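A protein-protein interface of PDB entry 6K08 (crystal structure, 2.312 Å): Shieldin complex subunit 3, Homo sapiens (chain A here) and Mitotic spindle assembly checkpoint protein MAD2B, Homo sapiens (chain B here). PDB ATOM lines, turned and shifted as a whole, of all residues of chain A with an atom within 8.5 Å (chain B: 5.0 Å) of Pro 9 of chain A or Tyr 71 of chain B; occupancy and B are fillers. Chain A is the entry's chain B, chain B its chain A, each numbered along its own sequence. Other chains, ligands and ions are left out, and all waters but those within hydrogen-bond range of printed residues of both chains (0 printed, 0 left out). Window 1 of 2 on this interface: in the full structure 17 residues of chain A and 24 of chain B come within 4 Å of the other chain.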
ATOM      1  N   PRO A   6     -27.365  24.485   5.173  1.00  0.00           N
ATOM      2  CA  PRO A   6     -28.173  23.346   4.722  1.00  0.00           C
ATOM      3  C   PRO A   6     -28.453  22.342   5.838  1.00  0.00           C
ATOM      4  O   PRO A   6     -27.997  22.476   6.972  1.00  0.00           O
ATOM      5  CB  PRO A   6     -27.296  22.730   3.632  1.00  0.00           C
ATOM      6  CG  PRO A   6     -25.904  22.997   4.108  1.00  0.00           C
ATOM      7  CD  PRO A   6     -25.948  24.344   4.791  1.00  0.00           C
ATOM      8  N   LEU A   7     -29.222  21.314   5.480  1.00  0.00           N
ATOM      9  CA  LEU A   7     -29.560  20.199   6.354  1.00  0.00           C
ATOM     10  C   LEU A   7     -28.667  18.997   6.061  1.00  0.00           C
ATOM     11  O   LEU A   7     -28.290  18.750   4.912  1.00  0.00           O
ATOM     12  CB  LEU A   7     -31.024  19.788   6.171  1.00  0.00           C
ATOM     13  CG  LEU A   7     -32.146  20.753   6.559  1.00  0.00           C
ATOM     14  CD1 LEU A   7     -33.441  20.368   5.866  1.00  0.00           C
ATOM     15  CD2 LEU A   7     -32.342  20.744   8.056  1.00  0.00           C
ATOM     16  N   ARG A   8     -28.362  18.229   7.102  1.00  0.00           N
ATOM     17  CA  ARG A   8     -27.607  16.995   6.952  1.00  0.00           C
ATOM     18  C   ARG A   8     -28.212  15.911   7.835  1.00  0.00           C
ATOM     19  O   ARG A   8     -28.915  16.209   8.808  1.00  0.00           O
ATOM     20  CB  ARG A   8     -26.120  17.196   7.282  1.00  0.00           C
ATOM     21  CG  ARG A   8     -25.792  17.334   8.749  1.00  0.00           C
ATOM     22  CD  ARG A   8     -24.344  16.945   8.972  1.00  0.00           C
ATOM     23  NE  ARG A   8     -23.818  17.359  10.264  1.00  0.00           N
ATOM     24  CZ  ARG A   8     -22.820  16.740  10.883  1.00  0.00           C
ATOM     25  NH1 ARG A   8     -22.260  15.673  10.330  1.00  0.00           N
ATOM     26  NH2 ARG A   8     -22.384  17.185  12.053  1.00  0.00           N
ATOM     27  N   PRO A   9     -27.994  14.638   7.485  1.00  0.00           N
ATOM     28  CA  PRO A   9     -28.286  13.547   8.424  1.00  0.00           C
ATOM     29  C   PRO A   9     -27.413  13.676   9.658  1.00  0.00           C
ATOM     30  O   PRO A   9     -26.221  13.980   9.565  1.00  0.00           O
ATOM     31  CB  PRO A   9     -27.942  12.281   7.622  1.00  0.00           C
ATOM     32  CG  PRO A   9     -27.928  12.722   6.181  1.00  0.00           C
ATOM     33  CD  PRO A   9     -27.461  14.135   6.210  1.00  0.00           C
ATOM     34  N   LYS A  10     -28.025  13.474  10.825  1.00  0.00           N
ATOM     35  CA  LYS A  10     -27.250  13.450  12.058  1.00  0.00           C
ATOM     36  C   LYS A  10     -26.419  12.178  12.159  1.00  0.00           C
ATOM     37  O   LYS A  10     -25.367  12.171  12.810  1.00  0.00           O
ATOM     38  CB  LYS A  10     -28.183  13.580  13.261  1.00  0.00           C
ATOM     39  CG  LYS A  10     -27.469  13.655  14.595  1.00  0.00           C
ATOM     40  CD  LYS A  10     -28.435  13.946  15.727  1.00  0.00           C
ATOM     41  CE  LYS A  10     -28.093  13.120  16.956  1.00  0.00           C
ATOM     42  NZ  LYS A  10     -28.220  13.911  18.209  1.00  0.00           N
ATOM     43  N   ARG A  11     -26.865  11.103  11.516  1.00  0.00           N
ATOM     44  CA  ARG A  11     -26.115   9.857  11.508  1.00  0.00           C
ATOM     45  C   ARG A  11     -25.029   9.903  10.441  1.00  0.00           C
ATOM     46  O   ARG A  11     -25.258  10.360   9.317  1.00  0.00           O
ATOM     47  CB  ARG A  11     -27.052   8.674  11.261  1.00  0.00           C
ATOM     48  N   SER A  12     -23.841   9.440  10.804  1.00  0.00           N
ATOM     49  CA  SER A  12     -22.751   9.387   9.846  1.00  0.00           C
ATOM     50  C   SER A  12     -22.823   8.090   9.045  1.00  0.00           C
ATOM     51  O   SER A  12     -23.370   7.089   9.520  1.00  0.00           O
ATOM     52  CB  SER A  12     -21.404   9.483  10.562  1.00  0.00           C
ATOM     53  OG  SER A  12     -21.123   8.309  11.307  1.00  0.00           O
ATOM     54  N   PRO A  13     -22.294   8.082   7.824  1.00  0.00           N
ATOM     55  CA  PRO A  13     -22.235   6.839   7.050  1.00  0.00           C
ATOM     56  C   PRO A  13     -21.409   5.794   7.777  1.00  0.00           C
ATOM     57  O   PRO A  13     -20.568   6.136   8.622  1.00  0.00           O
ATOM     58  CB  PRO A  13     -21.562   7.268   5.737  1.00  0.00           C
ATOM     59  CG  PRO A  13     -20.868   8.548   6.059  1.00  0.00           C
ATOM     60  CD  PRO A  13     -21.746   9.218   7.068  1.00  0.00           C
ATOM     61  N   PRO A  14     -21.615   4.514   7.482  1.00  0.00           N
ATOM     62  CA  PRO A  14     -20.866   3.476   8.192  1.00  0.00           C
ATOM     63  C   PRO A  14     -19.397   3.485   7.811  1.00  0.00           C
ATOM     64  O   PRO A  14     -19.011   3.904   6.715  1.00  0.00           O
ATOM     65  CB  PRO A  14     -21.547   2.180   7.743  1.00  0.00           C
ATOM     66  CG  PRO A  14     -22.064   2.500   6.386  1.00  0.00           C
ATOM     67  CD  PRO A  14     -22.505   3.942   6.456  1.00  0.00           C
ATOM     68  N   GLU B  67     -25.203  -2.128   4.881  1.00  0.00           N
ATOM     69  CA  GLU B  67     -25.478  -0.980   5.738  1.00  0.00           C
ATOM     70  C   GLU B  67     -25.119   0.340   5.071  1.00  0.00           C
ATOM     71  O   GLU B  67     -25.757   1.360   5.353  1.00  0.00           O
ATOM     72  CB  GLU B  67     -24.745  -1.119   7.073  1.00  0.00           C
ATOM     73  CG  GLU B  67     -25.672  -1.447   8.239  1.00  0.00           C
ATOM     74  CD  GLU B  67     -26.893  -0.541   8.295  1.00  0.00           C
ATOM     75  OE1 GLU B  67     -26.746   0.683   8.094  1.00  0.00           O
ATOM     76  OE2 GLU B  67     -28.006  -1.059   8.534  1.00  0.00           O
ATOM     77  N   LEU B  68     -24.112   0.353   4.195  1.00  0.00           N
ATOM     78  CA  LEU B  68     -23.879   1.546   3.388  1.00  0.00           C
ATOM     79  C   LEU B  68     -25.037   1.782   2.431  1.00  0.00           C
ATOM     80  O   LEU B  68     -25.485   2.920   2.250  1.00  0.00           O
ATOM     81  CB  LEU B  68     -22.567   1.425   2.613  1.00  0.00           C
ATOM     82  CG  LEU B  68     -22.329   2.582   1.641  1.00  0.00           C
ATOM     83  CD1 LEU B  68     -22.252   3.902   2.395  1.00  0.00           C
ATOM     84  CD2 LEU B  68     -21.078   2.361   0.803  1.00  0.00           C
ATOM     85  N   ASN B  69     -25.540   0.712   1.812  1.00  0.00           N
ATOM     86  CA  ASN B  69     -26.666   0.844   0.894  1.00  0.00           C
ATOM     87  C   ASN B  69     -27.912   1.339   1.617  1.00  0.00           C
ATOM     88  O   ASN B  69     -28.643   2.188   1.097  1.00  0.00           O
ATOM     89  CB  ASN B  69     -26.938  -0.491   0.205  1.00  0.00           C
ATOM     90  CG  ASN B  69     -25.815  -0.903  -0.723  1.00  0.00           C
ATOM     91  OD1 ASN B  69     -24.855  -0.159  -0.919  1.00  0.00           O
ATOM     92  ND2 ASN B  69     -25.927  -2.095  -1.297  1.00  0.00           N
ATOM     93  N   GLN B  70     -28.170   0.818   2.820  1.00  0.00           N
ATOM     94  CA  GLN B  70     -29.319   1.284   3.588  1.00  0.00           C
ATOM     95  C   GLN B  70     -29.161   2.740   4.001  1.00  0.00           C
ATOM     96  O   GLN B  70     -30.154   3.468   4.104  1.00  0.00           O
ATOM     97  CB  GLN B  70     -29.527   0.404   4.821  1.00  0.00           C
ATOM     98  CG  GLN B  70     -30.847   0.651   5.535  1.00  0.00           C
ATOM     99  CD  GLN B  70     -32.046   0.437   4.632  1.00  0.00           C
ATOM    100  OE1 GLN B  70     -32.220  -0.638   4.058  1.00  0.00           O
ATOM    101  NE2 GLN B  70     -32.879   1.464   4.498  1.00  0.00           N
ATOM    102  N   TYR B  71     -27.923   3.185   4.235  1.00  0.00           N
ATOM    103  CA  TYR B  71     -27.703   4.574   4.621  1.00  0.00           C
ATOM    104  C   TYR B  71     -28.026   5.523   3.474  1.00  0.00           C
ATOM    105  O   TYR B  71     -28.616   6.588   3.691  1.00  0.00           O
ATOM    106  CB  TYR B  71     -26.261   4.767   5.091  1.00  0.00           C
ATOM    107  CG  TYR B  71     -25.958   6.170   5.564  1.00  0.00           C
ATOM    108  CD1 TYR B  71     -25.453   7.126   4.690  1.00  0.00           C
ATOM    109  CD2 TYR B  71     -26.182   6.541   6.882  1.00  0.00           C
ATOM    110  CE1 TYR B  71     -25.179   8.410   5.118  1.00  0.00           C
ATOM    111  CE2 TYR B  71     -25.910   7.824   7.320  1.00  0.00           C
ATOM    112  CZ  TYR B  71     -25.408   8.753   6.433  1.00  0.00           C
ATOM    113  OH  TYR B  71     -25.135  10.032   6.861  1.00  0.00           O
ATOM    114  N   ILE B  72     -27.645   5.159   2.248  1.00  0.00           N
ATOM    115  CA  ILE B  72     -27.948   6.006   1.099  1.00  0.00           C
ATOM    116  C   ILE B  72     -29.446   6.012   0.820  1.00  0.00           C
ATOM    117  O   ILE B  72     -30.021   7.050   0.472  1.00  0.00           O
ATOM    118  CB  ILE B  72     -27.140   5.546  -0.128  1.00  0.00           C
ATOM    119  CG1 ILE B  72     -25.643   5.566   0.183  1.00  0.00           C
ATOM    120  CG2 ILE B  72     -27.440   6.426  -1.335  1.00  0.00           C
ATOM    121  CD1 ILE B  72     -24.807   4.779  -0.796  1.00  0.00           C
ATOM    122  N   GLN B  73     -30.102   4.860   0.979  1.00  0.00           N
ATOM    123  CA  GLN B  73     -31.542   4.785   0.755  1.00  0.00           C
ATOM    124  C   GLN B  73     -32.299   5.654   1.752  1.00  0.00           C
ATOM    125  O   GLN B  73     -33.192   6.421   1.374  1.00  0.00           O
ATOM    126  CB  GLN B  73     -32.013   3.333   0.844  1.00  0.00           C
ATOM    127  CG  GLN B  73     -31.748   2.510  -0.405  1.00  0.00           C
ATOM    128  CD  GLN B  73     -32.172   1.063  -0.248  1.00  0.00           C
ATOM    129  OE1 GLN B  73     -33.171   0.762   0.407  1.00  0.00           O
ATOM    130  NE2 GLN B  73     -31.412   0.155  -0.851  1.00  0.00           N
ATOM    131  N   ASP B  74     -31.951   5.543   3.038  1.00  0.00           N
ATOM    132  CA  ASP B  74     -32.609   6.349   4.061  1.00  0.00           C
ATOM    133  C   ASP B  74     -32.416   7.838   3.800  1.00  0.00           C
ATOM    134  O   ASP B  74     -33.348   8.631   3.975  1.00  0.00           O
ATOM    135  CB  ASP B  74     -32.078   5.974   5.445  1.00  0.00           C
ATOM    136  CG  ASP B  74     -32.465   4.567   5.861  1.00  0.00           C
ATOM    137  OD1 ASP B  74     -33.434   4.019   5.293  1.00  0.00           O
ATOM    138  OD2 ASP B  74     -31.803   4.007   6.760  1.00  0.00           O
ATOM    139  N   THR B  75     -31.212   8.235   3.381  1.00  0.00           N
ATOM    140  CA  THR B  75     -30.965   9.635   3.049  1.00  0.00           C
ATOM    141  C   THR B  75     -31.893  10.101   1.934  1.00  0.00           C
ATOM    142  O   THR B  75     -32.534  11.153   2.040  1.00  0.00           O
ATOM    143  CB  THR B  75     -29.501   9.830   2.647  1.00  0.00           C
ATOM    144  OG1 THR B  75     -28.646   9.319   3.678  1.00  0.00           O
ATOM    145  CG2 THR B  75     -29.197  11.307   2.426  1.00  0.00           C
ATOM    146  N   PHE B 154     -17.734  10.836   3.733  1.00  0.00           N
ATOM    147  CA  PHE B 154     -18.662  11.628   2.942  1.00  0.00           C
ATOM    148  C   PHE B 154     -19.894  11.998   3.760  1.00  0.00           C
ATOM    149  O   PHE B 154     -20.142  11.462   4.843  1.00  0.00           O
ATOM    150  CB  PHE B 154     -19.059  10.902   1.645  1.00  0.00           C
ATOM    151  CG  PHE B 154     -20.203   9.941   1.799  1.00  0.00           C
ATOM    152  CD1 PHE B 154     -19.988   8.654   2.263  1.00  0.00           C
ATOM    153  CD2 PHE B 154     -21.492  10.316   1.453  1.00  0.00           C
ATOM    154  CE1 PHE B 154     -21.038   7.766   2.391  1.00  0.00           C
ATOM    155  CE2 PHE B 154     -22.545   9.433   1.583  1.00  0.00           C
ATOM    156  CZ  PHE B 154     -22.319   8.156   2.053  1.00  0.00           C
ATOM    157  N   THR B 155     -20.657  12.945   3.216  1.00  0.00           N
ATOM    158  CA  THR B 155     -21.848  13.491   3.848  1.00  0.00           C
ATOM    159  C   THR B 155     -22.736  14.048   2.741  1.00  0.00           C
ATOM    160  O   THR B 155     -22.245  14.443   1.680  1.00  0.00           O
ATOM    161  CB  THR B 155     -21.480  14.577   4.879  1.00  0.00           C
ATOM    162  OG1 THR B 155     -20.753  13.984   5.962  1.00  0.00           O
ATOM    163  CG2 THR B 155     -22.718  15.262   5.451  1.00  0.00           C
ATOM    164  N   VAL B 156     -24.048  14.041   2.977  1.00  0.00           N
ATOM    165  CA  VAL B 156     -25.021  14.629   2.062  1.00  0.00           C
ATOM    166  C   VAL B 156     -25.675  15.819   2.754  1.00  0.00           C
ATOM    167  O   VAL B 156     -26.126  15.707   3.900  1.00  0.00           O
ATOM    168  CB  VAL B 156     -26.082  13.606   1.610  1.00  0.00           C
ATOM    169  CG1 VAL B 156     -27.021  14.239   0.588  1.00  0.00           C
ATOM    170  CG2 VAL B 156     -25.414  12.370   1.026  1.00  0.00           C
ATOM    171  N   PHE B 177     -33.615   8.028  12.003  1.00  0.00           N
ATOM    172  CA  PHE B 177     -32.687   8.608  11.032  1.00  0.00           C
ATOM    173  C   PHE B 177     -32.898  10.117  11.008  1.00  0.00           C
ATOM    174  O   PHE B 177     -33.407  10.674  10.027  1.00  0.00           O
ATOM    175  CB  PHE B 177     -32.880   8.000   9.642  1.00  0.00           C
ATOM    176  CG  PHE B 177     -31.709   8.213   8.717  1.00  0.00           C
ATOM    177  CD1 PHE B 177     -30.636   7.335   8.725  1.00  0.00           C
ATOM    178  CD2 PHE B 177     -31.682   9.288   7.842  1.00  0.00           C
ATOM    179  CE1 PHE B 177     -29.558   7.526   7.878  1.00  0.00           C
ATOM    180  CE2 PHE B 177     -30.606   9.484   6.993  1.00  0.00           C
ATOM    181  CZ  PHE B 177     -29.542   8.601   7.011  1.00  0.00           C
ATOM    182  N   PRO B 178     -32.512  10.812  12.074  1.00  0.00           N
ATOM    183  CA  PRO B 178     -32.803  12.244  12.163  1.00  0.00           C
ATOM    184  C   PRO B 178     -31.879  13.070  11.282  1.00  0.00           C
ATOM    185  O   PRO B 178     -30.819  12.623  10.838  1.00  0.00           O
ATOM    186  CB  PRO B 178     -32.577  12.558  13.645  1.00  0.00           C
ATOM    187  CG  PRO B 178     -31.541  11.574  14.065  1.00  0.00           C
ATOM    188  CD  PRO B 178     -31.793  10.320  13.264  1.00  0.00           C
ATOM    189  N   TRP B 179     -32.314  14.298  11.029  1.00  0.00           N
ATOM    190  CA  TRP B 179     -31.529  15.305  10.335  1.00  0.00           C
ATOM    191  C   TRP B 179     -31.214  16.444  11.296  1.00  0.00           C
ATOM    192  O   TRP B 179     -31.784  16.548  12.383  1.00  0.00           O
ATOM    193  CB  TRP B 179     -32.275  15.824   9.098  1.00  0.00           C
ATOM    194  CG  TRP B 179     -32.392  14.809   8.001  1.00  0.00           C
ATOM    195  CD1 TRP B 179     -33.073  13.627   8.049  1.00  0.00           C
ATOM    196  CD2 TRP B 179     -31.814  14.885   6.691  1.00  0.00           C
ATOM    197  NE1 TRP B 179     -32.954  12.962   6.854  1.00  0.00           N
ATOM    198  CE2 TRP B 179     -32.186  13.713   6.003  1.00  0.00           C
ATOM    199  CE3 TRP B 179     -31.019  15.829   6.034  1.00  0.00           C
ATOM    200  CZ2 TRP B 179     -31.789  13.460   4.691  1.00  0.00           C
ATOM    201  CZ3 TRP B 179     -30.626  15.575   4.731  1.00  0.00           C
ATOM    202  CH2 TRP B 179     -31.012  14.401   4.075  1.00  0.00           C
ATOM    203  N   ILE B 180     -30.279  17.302  10.887  1.00  0.00           N
ATOM    204  CA  ILE B 180     -29.865  18.459  11.673  1.00  0.00           C
ATOM    205  C   ILE B 180     -29.520  19.595  10.719  1.00  0.00           C
ATOM    206  O   ILE B 180     -29.479  19.425   9.498  1.00  0.00           O
ATOM    207  CB  ILE B 180     -28.646  18.165  12.581  1.00  0.00           C
ATOM    208  CG1 ILE B 180     -27.470  17.663  11.746  1.00  0.00           C
ATOM    209  CG2 ILE B 180     -28.996  17.181  13.684  1.00  0.00           C
ATOM    210  CD1 ILE B 180     -26.324  17.102  12.559  1.00  0.00           C
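The side-chain hydroxyl of Tyr 71 of chain B sits at hydrogen-bond distance from the backbone carbonyl oxygen of Arg 11 of chain A (2.5 Å).
The backbone carbonyl oxygen of Arg 8 of chain A sits at hydrogen-bond distance from the backbone NH of Ile 180 of chain B, at 2.7 Å.
The backbone NH (N) of Lys 10 of chain A lies within hydrogen-bond range of the backbone carbonyl oxygen (O) of Pro 178 of chain B, 2.9 Å away.
O of Tyr 71 of chain B is in hydrogen-bond range of OG1 of Thr 75 of chain B (2.7 Å).
Among the printed residues, merely in contact across the chains: Pro 9 of chain A with Val 156 of chain B (3.1 Å), Arg 8 of chain A with Trp 179 of chain B (3.2 Å), Leu 7 of chain A with Ile 180 of chain B (3.2 Å), Pro 13 of chain A with Phe 154 of chain B (3.2 Å), Ser 12 of chain A with Tyr 71 of chain B (3.4 Å), Pro 13 of chain A with Tyr 71 of chain B (3.5 Å), Pro 9 of chain A with Trp 179 of chain B (3.6 Å), Pro 9 of chain A with Pro 178 of chain B (3.6 Å), Arg 8 of chain A with Val 156 of chain B (3.6 Å), Pro 14 of chain A with Leu 68 of chain B (3.6 Å), Pro 9 of chain A with Tyr 71 of chain B (3.7 Å), Lys 10 of chain A with Ile 180 of chain B (3.7 Å), Leu 7 of chain A with Val 156 of chain B (3.9 Å), Pro 9 of chain A with Phe 177 of chain B (3.9 Å), Leu 7 of chain A with Trp 179 of chain B (3.9 Å), Pro 14 of chain A with Glu 67 of chain B (3.97 Å) and Lys 10 of chain A with Trp 179 of chain B (3.98 Å).
Of chain B, only Tyr 71, Val 156, Phe 177, Pro 178 and Trp 179 come within 4 Å of Pro 9 of chain A.
Of the printed residues of chain B, Lys 10 of chain A touches Pro 178 (2.9 Å), Trp 179 (3.98 Å) and Ile 180 (3.7 Å).
Of the printed residues of chain B, Ser 12 of chain A touches Tyr 71.
Printed residues of chain B within 4 Å of Pro 13 of chain A: Tyr 71 and Phe 154.
Of chain A, only Pro 9, Arg 11, Ser 12 and Pro 13 come within 4 Å of Tyr 71 of chain B.
Thr 75 of chain B touches none of the printed residues of chain A.
Thr 155 of chain B touches none of the printed residues of chain A.
The nearest residue of chain B that does not touch Pro 9 of chain A is Thr 75 of chain B (4.2 Å).
The nearest printed residue of chain A that does not touch Trp 179 of chain B is Arg 11 of chain A (6.3 Å).
Of the 9 printed residues of chain A, 8 touch a printed residue of chain B.
Hydrophobic or aromatic side chains of chain A that line the printed part of chain B: Leu 7, Pro 9, Pro 13 and Pro 14.
Of the 16 printed residues of chain B, 9 touch a printed residue of chain A.
Printed residues of chain B that touch a printed residue of chain A: Glu 67, Leu 68, Tyr 71, Phe 154, Val 156, Phe 177, Pro 178, Trp 179 and Ile 180.
Hydrophobic or aromatic side chains of chain B within 4 Å of the printed part of chain A: Leu 68, Tyr 71, Phe 154, Phe 177, Pro 178, Trp 179 and Ile 180.
Among the printed residues, 20 pairs touch across the chains.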
